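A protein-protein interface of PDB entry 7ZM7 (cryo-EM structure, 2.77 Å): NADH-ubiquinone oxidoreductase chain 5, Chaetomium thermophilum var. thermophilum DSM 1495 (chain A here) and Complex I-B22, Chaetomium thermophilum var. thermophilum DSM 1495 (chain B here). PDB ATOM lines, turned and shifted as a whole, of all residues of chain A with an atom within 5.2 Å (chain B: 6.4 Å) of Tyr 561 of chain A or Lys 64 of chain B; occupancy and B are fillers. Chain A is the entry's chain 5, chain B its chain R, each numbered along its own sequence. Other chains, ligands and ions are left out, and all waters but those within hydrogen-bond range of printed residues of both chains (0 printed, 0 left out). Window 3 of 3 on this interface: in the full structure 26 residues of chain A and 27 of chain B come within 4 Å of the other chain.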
ATOM      1  N   PHE A 554      16.472  -3.056  24.236  1.00  0.00           N
ATOM      2  CA  PHE A 554      17.805  -2.642  23.834  1.00  0.00           C
ATOM      3  C   PHE A 554      17.746  -1.484  22.852  1.00  0.00           C
ATOM      4  O   PHE A 554      18.442  -0.481  23.022  1.00  0.00           O
ATOM      5  CB  PHE A 554      18.544  -3.829  23.227  1.00  0.00           C
ATOM      6  CG  PHE A 554      20.025  -3.761  23.387  1.00  0.00           C
ATOM      7  CD1 PHE A 554      20.792  -3.003  22.524  1.00  0.00           C
ATOM      8  CD2 PHE A 554      20.652  -4.455  24.404  1.00  0.00           C
ATOM      9  CE1 PHE A 554      22.157  -2.939  22.673  1.00  0.00           C
ATOM     10  CE2 PHE A 554      22.017  -4.396  24.559  1.00  0.00           C
ATOM     11  CZ  PHE A 554      22.772  -3.636  23.690  1.00  0.00           C
ATOM     12  N   LYS A 555      16.897  -1.595  21.835  1.00  0.00           N
ATOM     13  CA  LYS A 555      16.794  -0.540  20.838  1.00  0.00           C
ATOM     14  C   LYS A 555      16.293   0.753  21.457  1.00  0.00           C
ATOM     15  O   LYS A 555      16.706   1.844  21.053  1.00  0.00           O
ATOM     16  CB  LYS A 555      15.868  -0.979  19.707  1.00  0.00           C
ATOM     17  CG  LYS A 555      16.517  -1.896  18.693  1.00  0.00           C
ATOM     18  CD  LYS A 555      15.645  -2.030  17.466  1.00  0.00           C
ATOM     19  CE  LYS A 555      15.205  -3.458  17.276  1.00  0.00           C
ATOM     20  NZ  LYS A 555      14.117  -3.544  16.276  1.00  0.00           N
ATOM     21  N   SER A 557      16.493   1.407  24.807  1.00  0.00           N
ATOM     22  CA  SER A 557      17.427   1.993  25.747  1.00  0.00           C
ATOM     23  C   SER A 557      18.262   3.045  25.025  1.00  0.00           C
ATOM     24  O   SER A 557      18.488   2.975  23.817  1.00  0.00           O
ATOM     25  CB  SER A 557      18.346   0.938  26.353  1.00  0.00           C
ATOM     26  OG  SER A 557      19.400   0.622  25.472  1.00  0.00           O
ATOM     27  N   ARG A 558      18.699   4.048  25.770  1.00  0.00           N
ATOM     28  CA  ARG A 558      19.577   5.026  25.154  1.00  0.00           C
ATOM     29  C   ARG A 558      20.947   4.439  24.857  1.00  0.00           C
ATOM     30  O   ARG A 558      21.547   4.773  23.834  1.00  0.00           O
ATOM     31  CB  ARG A 558      19.693   6.267  26.037  1.00  0.00           C
ATOM     32  CG  ARG A 558      20.616   7.319  25.470  1.00  0.00           C
ATOM     33  CD  ARG A 558      20.038   7.860  24.184  1.00  0.00           C
ATOM     34  NE  ARG A 558      18.788   8.572  24.400  1.00  0.00           N
ATOM     35  CZ  ARG A 558      17.964   8.931  23.425  1.00  0.00           C
ATOM     36  NH1 ARG A 558      16.844   9.577  23.708  1.00  0.00           N
ATOM     37  NH2 ARG A 558      18.250   8.629  22.168  1.00  0.00           N
ATOM     38  N   PHE A 559      21.451   3.564  25.725  1.00  0.00           N
ATOM     39  CA  PHE A 559      22.732   2.924  25.454  1.00  0.00           C
ATOM     40  C   PHE A 559      22.663   2.098  24.181  1.00  0.00           C
ATOM     41  O   PHE A 559      23.608   2.087  23.387  1.00  0.00           O
ATOM     42  CB  PHE A 559      23.148   2.051  26.636  1.00  0.00           C
ATOM     43  CG  PHE A 559      24.335   1.180  26.354  1.00  0.00           C
ATOM     44  CD1 PHE A 559      25.611   1.708  26.363  1.00  0.00           C
ATOM     45  CD2 PHE A 559      24.175  -0.163  26.074  1.00  0.00           C
ATOM     46  CE1 PHE A 559      26.704   0.912  26.104  1.00  0.00           C
ATOM     47  CE2 PHE A 559      25.264  -0.962  25.814  1.00  0.00           C
ATOM     48  CZ  PHE A 559      26.531  -0.424  25.829  1.00  0.00           C
ATOM     49  N   GLY A 560      21.552   1.394  23.974  1.00  0.00           N
ATOM     50  CA  GLY A 560      21.405   0.589  22.776  1.00  0.00           C
ATOM     51  C   GLY A 560      21.004   1.390  21.554  1.00  0.00           C
ATOM     52  O   GLY A 560      21.305   1.004  20.426  1.00  0.00           O
ATOM     53  N   TYR A 561      20.300   2.504  21.753  1.00  0.00           N
ATOM     54  CA  TYR A 561      19.977   3.379  20.633  1.00  0.00           C
ATOM     55  C   TYR A 561      21.236   3.872  19.958  1.00  0.00           C
ATOM     56  O   TYR A 561      21.252   4.114  18.748  1.00  0.00           O
ATOM     57  CB  TYR A 561      19.145   4.560  21.119  1.00  0.00           C
ATOM     58  CG  TYR A 561      18.855   5.614  20.078  1.00  0.00           C
ATOM     59  CD1 TYR A 561      19.744   6.648  19.841  1.00  0.00           C
ATOM     60  CD2 TYR A 561      17.673   5.598  19.360  1.00  0.00           C
ATOM     61  CE1 TYR A 561      19.484   7.607  18.913  1.00  0.00           C
ATOM     62  CE2 TYR A 561      17.400   6.565  18.433  1.00  0.00           C
ATOM     63  CZ  TYR A 561      18.312   7.568  18.212  1.00  0.00           C
ATOM     64  OH  TYR A 561      18.066   8.542  17.281  1.00  0.00           O
ATOM     65  N   ASN A 562      22.302   4.037  20.730  1.00  0.00           N
ATOM     66  CA  ASN A 562      23.530   4.574  20.176  1.00  0.00           C
ATOM     67  C   ASN A 562      24.401   3.480  19.593  1.00  0.00           C
ATOM     68  O   ASN A 562      25.028   3.671  18.547  1.00  0.00           O
ATOM     69  CB  ASN A 562      24.273   5.340  21.252  1.00  0.00           C
ATOM     70  CG  ASN A 562      23.755   6.721  21.404  1.00  0.00           C
ATOM     71  OD1 ASN A 562      22.690   7.042  20.896  1.00  0.00           O
ATOM     72  ND2 ASN A 562      24.500   7.564  22.101  1.00  0.00           N
ATOM     73  N   ILE A 563      24.465   2.329  20.261  1.00  0.00           N
ATOM     74  CA  ILE A 563      25.263   1.235  19.735  1.00  0.00           C
ATOM     75  C   ILE A 563      24.637   0.718  18.454  1.00  0.00           C
ATOM     76  O   ILE A 563      25.343   0.315  17.525  1.00  0.00           O
ATOM     77  CB  ILE A 563      25.424   0.130  20.792  1.00  0.00           C
ATOM     78  CG1 ILE A 563      26.509  -0.859  20.376  1.00  0.00           C
ATOM     79  CG2 ILE A 563      24.141  -0.615  20.997  1.00  0.00           C
ATOM     80  CD1 ILE A 563      27.892  -0.251  20.341  1.00  0.00           C
ATOM     81  N   PHE A 564      23.306   0.743  18.376  1.00  0.00           N
ATOM     82  CA  PHE A 564      22.618   0.325  17.166  1.00  0.00           C
ATOM     83  C   PHE A 564      22.950   1.247  16.006  1.00  0.00           C
ATOM     84  O   PHE A 564      23.319   0.792  14.921  1.00  0.00           O
ATOM     85  CB  PHE A 564      21.115   0.299  17.424  1.00  0.00           C
ATOM     86  CG  PHE A 564      20.312  -0.236  16.288  1.00  0.00           C
ATOM     87  CD1 PHE A 564      20.077  -1.586  16.173  1.00  0.00           C
ATOM     88  CD2 PHE A 564      19.773   0.605  15.348  1.00  0.00           C
ATOM     89  CE1 PHE A 564      19.337  -2.076  15.140  1.00  0.00           C
ATOM     90  CE2 PHE A 564      19.034   0.107  14.308  1.00  0.00           C
ATOM     91  CZ  PHE A 564      18.808  -1.228  14.211  1.00  0.00           C
ATOM     92  N   GLY A 565      22.842   2.553  16.221  1.00  0.00           N
ATOM     93  CA  GLY A 565      23.070   3.485  15.136  1.00  0.00           C
ATOM     94  C   GLY A 565      24.528   3.671  14.781  1.00  0.00           C
ATOM     95  O   GLY A 565      24.843   4.200  13.718  1.00  0.00           O
ATOM     96  N   TRP B  21      11.285   0.717  14.776  1.00  0.00           N
ATOM     97  CA  TRP B  21      12.154   0.154  15.837  1.00  0.00           C
ATOM     98  C   TRP B  21      11.606  -1.176  16.338  1.00  0.00           C
ATOM     99  O   TRP B  21      12.384  -1.935  16.886  1.00  0.00           O
ATOM    100  CB  TRP B  21      12.362   1.172  16.950  1.00  0.00           C
ATOM    101  CG  TRP B  21      13.226   2.347  16.624  1.00  0.00           C
ATOM    102  CD1 TRP B  21      12.819   3.592  16.250  1.00  0.00           C
ATOM    103  CD2 TRP B  21      14.657   2.405  16.719  1.00  0.00           C
ATOM    104  NE1 TRP B  21      13.900   4.414  16.081  1.00  0.00           N
ATOM    105  CE2 TRP B  21      15.042   3.713  16.361  1.00  0.00           C
ATOM    106  CE3 TRP B  21      15.649   1.477  17.045  1.00  0.00           C
ATOM    107  CZ2 TRP B  21      16.376   4.106  16.320  1.00  0.00           C
ATOM    108  CZ3 TRP B  21      16.966   1.868  17.013  1.00  0.00           C
ATOM    109  CH2 TRP B  21      17.322   3.166  16.656  1.00  0.00           C
ATOM    110  N   GLU B  59       8.224  17.505  18.427  1.00  0.00           N
ATOM    111  CA  GLU B  59       9.148  17.525  17.307  1.00  0.00           C
ATOM    112  C   GLU B  59      10.541  17.132  17.754  1.00  0.00           C
ATOM    113  O   GLU B  59      11.377  16.771  16.919  1.00  0.00           O
ATOM    114  CB  GLU B  59       9.149  18.911  16.656  1.00  0.00           C
ATOM    115  CG  GLU B  59      10.006  19.028  15.408  1.00  0.00           C
ATOM    116  CD  GLU B  59       9.457  18.220  14.251  1.00  0.00           C
ATOM    117  OE1 GLU B  59       8.223  18.041  14.185  1.00  0.00           O
ATOM    118  OE2 GLU B  59      10.258  17.765  13.407  1.00  0.00           O
ATOM    119  N   LYS B  60      10.802  17.182  19.052  1.00  0.00           N
ATOM    120  CA  LYS B  60      12.102  16.795  19.571  1.00  0.00           C
ATOM    121  C   LYS B  60      12.223  15.294  19.762  1.00  0.00           C
ATOM    122  O   LYS B  60      13.300  14.736  19.555  1.00  0.00           O
ATOM    123  CB  LYS B  60      12.385  17.529  20.881  1.00  0.00           C
ATOM    124  CG  LYS B  60      12.594  19.004  20.681  1.00  0.00           C
ATOM    125  CD  LYS B  60      12.807  19.725  21.999  1.00  0.00           C
ATOM    126  CE  LYS B  60      14.158  19.377  22.604  1.00  0.00           C
ATOM    127  NZ  LYS B  60      15.278  19.923  21.789  1.00  0.00           N
ATOM    128  N   LEU B  61      11.145  14.616  20.146  1.00  0.00           N
ATOM    129  CA  LEU B  61      11.260  13.185  20.401  1.00  0.00           C
ATOM    130  C   LEU B  61      11.382  12.389  19.112  1.00  0.00           C
ATOM    131  O   LEU B  61      11.959  11.298  19.109  1.00  0.00           O
ATOM    132  CB  LEU B  61      10.082  12.677  21.222  1.00  0.00           C
ATOM    133  CG  LEU B  61       9.838  13.288  22.594  1.00  0.00           C
ATOM    134  CD1 LEU B  61       8.967  14.496  22.515  1.00  0.00           C
ATOM    135  CD2 LEU B  61       9.220  12.256  23.510  1.00  0.00           C
ATOM    136  N   LEU B  62      10.848  12.906  18.015  1.00  0.00           N
ATOM    137  CA  LEU B  62      10.966  12.178  16.763  1.00  0.00           C
ATOM    138  C   LEU B  62      12.394  12.193  16.242  1.00  0.00           C
ATOM    139  O   LEU B  62      12.802  11.255  15.552  1.00  0.00           O
ATOM    140  CB  LEU B  62      10.001  12.746  15.730  1.00  0.00           C
ATOM    141  CG  LEU B  62       8.546  12.807  16.179  1.00  0.00           C
ATOM    142  CD1 LEU B  62       7.653  12.933  14.980  1.00  0.00           C
ATOM    143  CD2 LEU B  62       8.170  11.582  16.966  1.00  0.00           C
ATOM    144  N   GLU B  63      13.166  13.230  16.557  1.00  0.00           N
ATOM    145  CA  GLU B  63      14.599  13.172  16.297  1.00  0.00           C
ATOM    146  C   GLU B  63      15.367  12.549  17.452  1.00  0.00           C
ATOM    147  O   GLU B  63      16.417  11.942  17.227  1.00  0.00           O
ATOM    148  CB  GLU B  63      15.138  14.569  15.984  1.00  0.00           C
ATOM    149  CG  GLU B  63      14.963  15.589  17.090  1.00  0.00           C
ATOM    150  CD  GLU B  63      16.141  15.627  18.045  1.00  0.00           C
ATOM    151  OE1 GLU B  63      17.245  15.195  17.650  1.00  0.00           O
ATOM    152  OE2 GLU B  63      15.961  16.078  19.194  1.00  0.00           O
ATOM    153  N   LYS B  64      14.857  12.667  18.679  1.00  0.00           N
ATOM    154  CA  LYS B  64      15.492  12.029  19.822  1.00  0.00           C
ATOM    155  C   LYS B  64      15.355  10.519  19.770  1.00  0.00           C
ATOM    156  O   LYS B  64      16.033   9.816  20.525  1.00  0.00           O
ATOM    157  CB  LYS B  64      14.893  12.575  21.121  1.00  0.00           C
ATOM    158  CG  LYS B  64      15.747  12.380  22.372  1.00  0.00           C
ATOM    159  CD  LYS B  64      15.174  13.170  23.539  1.00  0.00           C
ATOM    160  CE  LYS B  64      16.047  13.077  24.781  1.00  0.00           C
ATOM    161  NZ  LYS B  64      15.994  11.738  25.422  1.00  0.00           N
ATOM    162  N   TRP B  65      14.501  10.008  18.886  1.00  0.00           N
ATOM    163  CA  TRP B  65      14.358   8.576  18.667  1.00  0.00           C
ATOM    164  C   TRP B  65      14.366   8.229  17.187  1.00  0.00           C
ATOM    165  O   TRP B  65      13.852   7.181  16.801  1.00  0.00           O
ATOM    166  CB  TRP B  65      13.089   8.061  19.342  1.00  0.00           C
ATOM    167  CG  TRP B  65      13.220   8.131  20.812  1.00  0.00           C
ATOM    168  CD1 TRP B  65      12.611   9.012  21.650  1.00  0.00           C
ATOM    169  CD2 TRP B  65      14.052   7.313  21.627  1.00  0.00           C
ATOM    170  NE1 TRP B  65      12.999   8.784  22.939  1.00  0.00           N
ATOM    171  CE2 TRP B  65      13.890   7.748  22.954  1.00  0.00           C
ATOM    172  CE3 TRP B  65      14.916   6.250  21.367  1.00  0.00           C
ATOM    173  CZ2 TRP B  65      14.558   7.158  24.012  1.00  0.00           C
ATOM    174  CZ3 TRP B  65      15.574   5.664  22.425  1.00  0.00           C
ATOM    175  CH2 TRP B  65      15.392   6.117  23.727  1.00  0.00           C
ATOM    176  N   LYS B  66      14.948   9.078  16.354  1.00  0.00           N
ATOM    177  CA  LYS B  66      14.910   8.851  14.918  1.00  0.00           C
ATOM    178  C   LYS B  66      15.641   7.569  14.558  1.00  0.00           C
ATOM    179  O   LYS B  66      16.731   7.291  15.060  1.00  0.00           O
ATOM    180  CB  LYS B  66      15.518  10.035  14.169  1.00  0.00           C
ATOM    181  CG  LYS B  66      16.962  10.347  14.494  1.00  0.00           C
ATOM    182  CD  LYS B  66      17.509  11.369  13.510  1.00  0.00           C
ATOM    183  CE  LYS B  66      18.937  11.789  13.836  1.00  0.00           C
ATOM    184  NZ  LYS B  66      19.027  12.561  15.094  1.00  0.00           N
ATOM    185  N   HIS B  67      14.988   6.796  13.698  1.00  0.00           N
ATOM    186  CA  HIS B  67      15.601   5.535  13.237  1.00  0.00           C
ATOM    187  C   HIS B  67      16.791   5.881  12.325  1.00  0.00           C
ATOM    188  O   HIS B  67      16.646   6.828  11.528  1.00  0.00           O
ATOM    189  CB  HIS B  67      14.522   4.692  12.562  1.00  0.00           C
ATOM    190  CG  HIS B  67      14.844   3.235  12.533  1.00  0.00           C
ATOM    191  ND1 HIS B  67      15.637   2.670  11.556  1.00  0.00           N
ATOM    192  CD2 HIS B  67      14.492   2.227  13.359  1.00  0.00           C
ATOM    193  CE1 HIS B  67      15.757   1.377  11.781  1.00  0.00           C
ATOM    194  NE2 HIS B  67      15.065   1.080  12.881  1.00  0.00           N
ATOM    195  N   PRO B  68      17.963   5.204  12.398  1.00  0.00           N
ATOM    196  CA  PRO B  68      19.061   5.468  11.461  1.00  0.00           C
ATOM    197  C   PRO B  68      18.644   5.334  10.010  1.00  0.00           C
ATOM    198  O   PRO B  68      19.075   6.133   9.170  1.00  0.00           O
ATOM    199  CB  PRO B  68      20.099   4.416  11.848  1.00  0.00           C
ATOM    200  CG  PRO B  68      19.727   3.980  13.208  1.00  0.00           C
ATOM    201  CD  PRO B  68      18.268   4.084  13.294  1.00  0.00           C
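Among the printed residues, merely in contact across the chains: Arg 558 of chain A with Trp 65 of chain B (3.3 Å), Tyr 561 of chain A with Trp 21 of chain B (3.4 Å), Tyr 561 of chain A with Trp 65 of chain B (3.5 Å), Phe 564 of chain A with Trp 21 of chain B (3.5 Å), Tyr 561 of chain A with Glu 63 of chain B (3.8 Å), Gly 565 of chain A with Pro 68 of chain B (3.9 Å), Tyr 561 of chain A with Lys 64 of chain B (3.9 Å) and Phe 564 of chain A with Pro 68 of chain B (3.997 Å).
Of the printed residues of chain B, Lys 555 of chain A touches Trp 21. Printed residues of chain B within 4 Å of Arg 558 of chain A: Lys 64 (2.9 Å) and Trp 65 (3.3 Å). Tyr 561 of chain A touches just these residues of chain B: Trp 21, Glu 63, Lys 64, Trp 65 and Lys 66. Of the printed residues of chain B, Gly 565 of chain A touches Pro 68 (3.9 Å). Leu 61 of chain B touches none of the printed residues of chain A. Lys 64 of chain B touches just these residues of chain A: Arg 558 and Tyr 561. Of the printed residues of chain A, Trp 65 of chain B touches Arg 558 (3.3 Å) and Tyr 561 (3.5 Å). The nearest printed residue of chain A that does not touch Lys 64 of chain B is Asn 562 of chain A (7.2 Å).
The side-chain amino group of Lys 555 of chain A sits at hydrogen-bond distance from the backbone carbonyl oxygen of Trp 21 of chain B (2.4 Å). The backbone carbonyl oxygen (O) of Lys 66 of chain B sits at hydrogen-bond distance from the side-chain hydroxyl (OH) of Tyr 561 of chain A. The guanidinium group of Arg 558 of chain A is in hydrogen-bond range of the backbone carbonyl oxygen of Lys 64 of chain B (3.0 Å).
The backbone carbonyl oxygen (O) of Glu 63 of chain B lies close to the side-chain amino group (NZ) of Lys 66 of chain B. O of Trp 65 of chain B is in hydrogen-bond range of NE1 of Trp 21 of chain B (2.9 Å).
Printed residues of chain B that touch a printed residue of chain A: Trp 21, Glu 63, Lys 64, Trp 65, Lys 66 and Pro 68. Hydrophobic or aromatic side chains of chain B within 4 Å of the printed part of chain A: Trp 21, Trp 65 and Pro 68. Along chain B the printed residues that touch a printed residue of chain A span positions 21 to 68. Among the printed residues, 11 pairs touch across the chains. Among the printed residues, no Asp or Glu carboxylate lies within 4 Å of a Lys or Arg side-chain nitrogen of the other chain.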
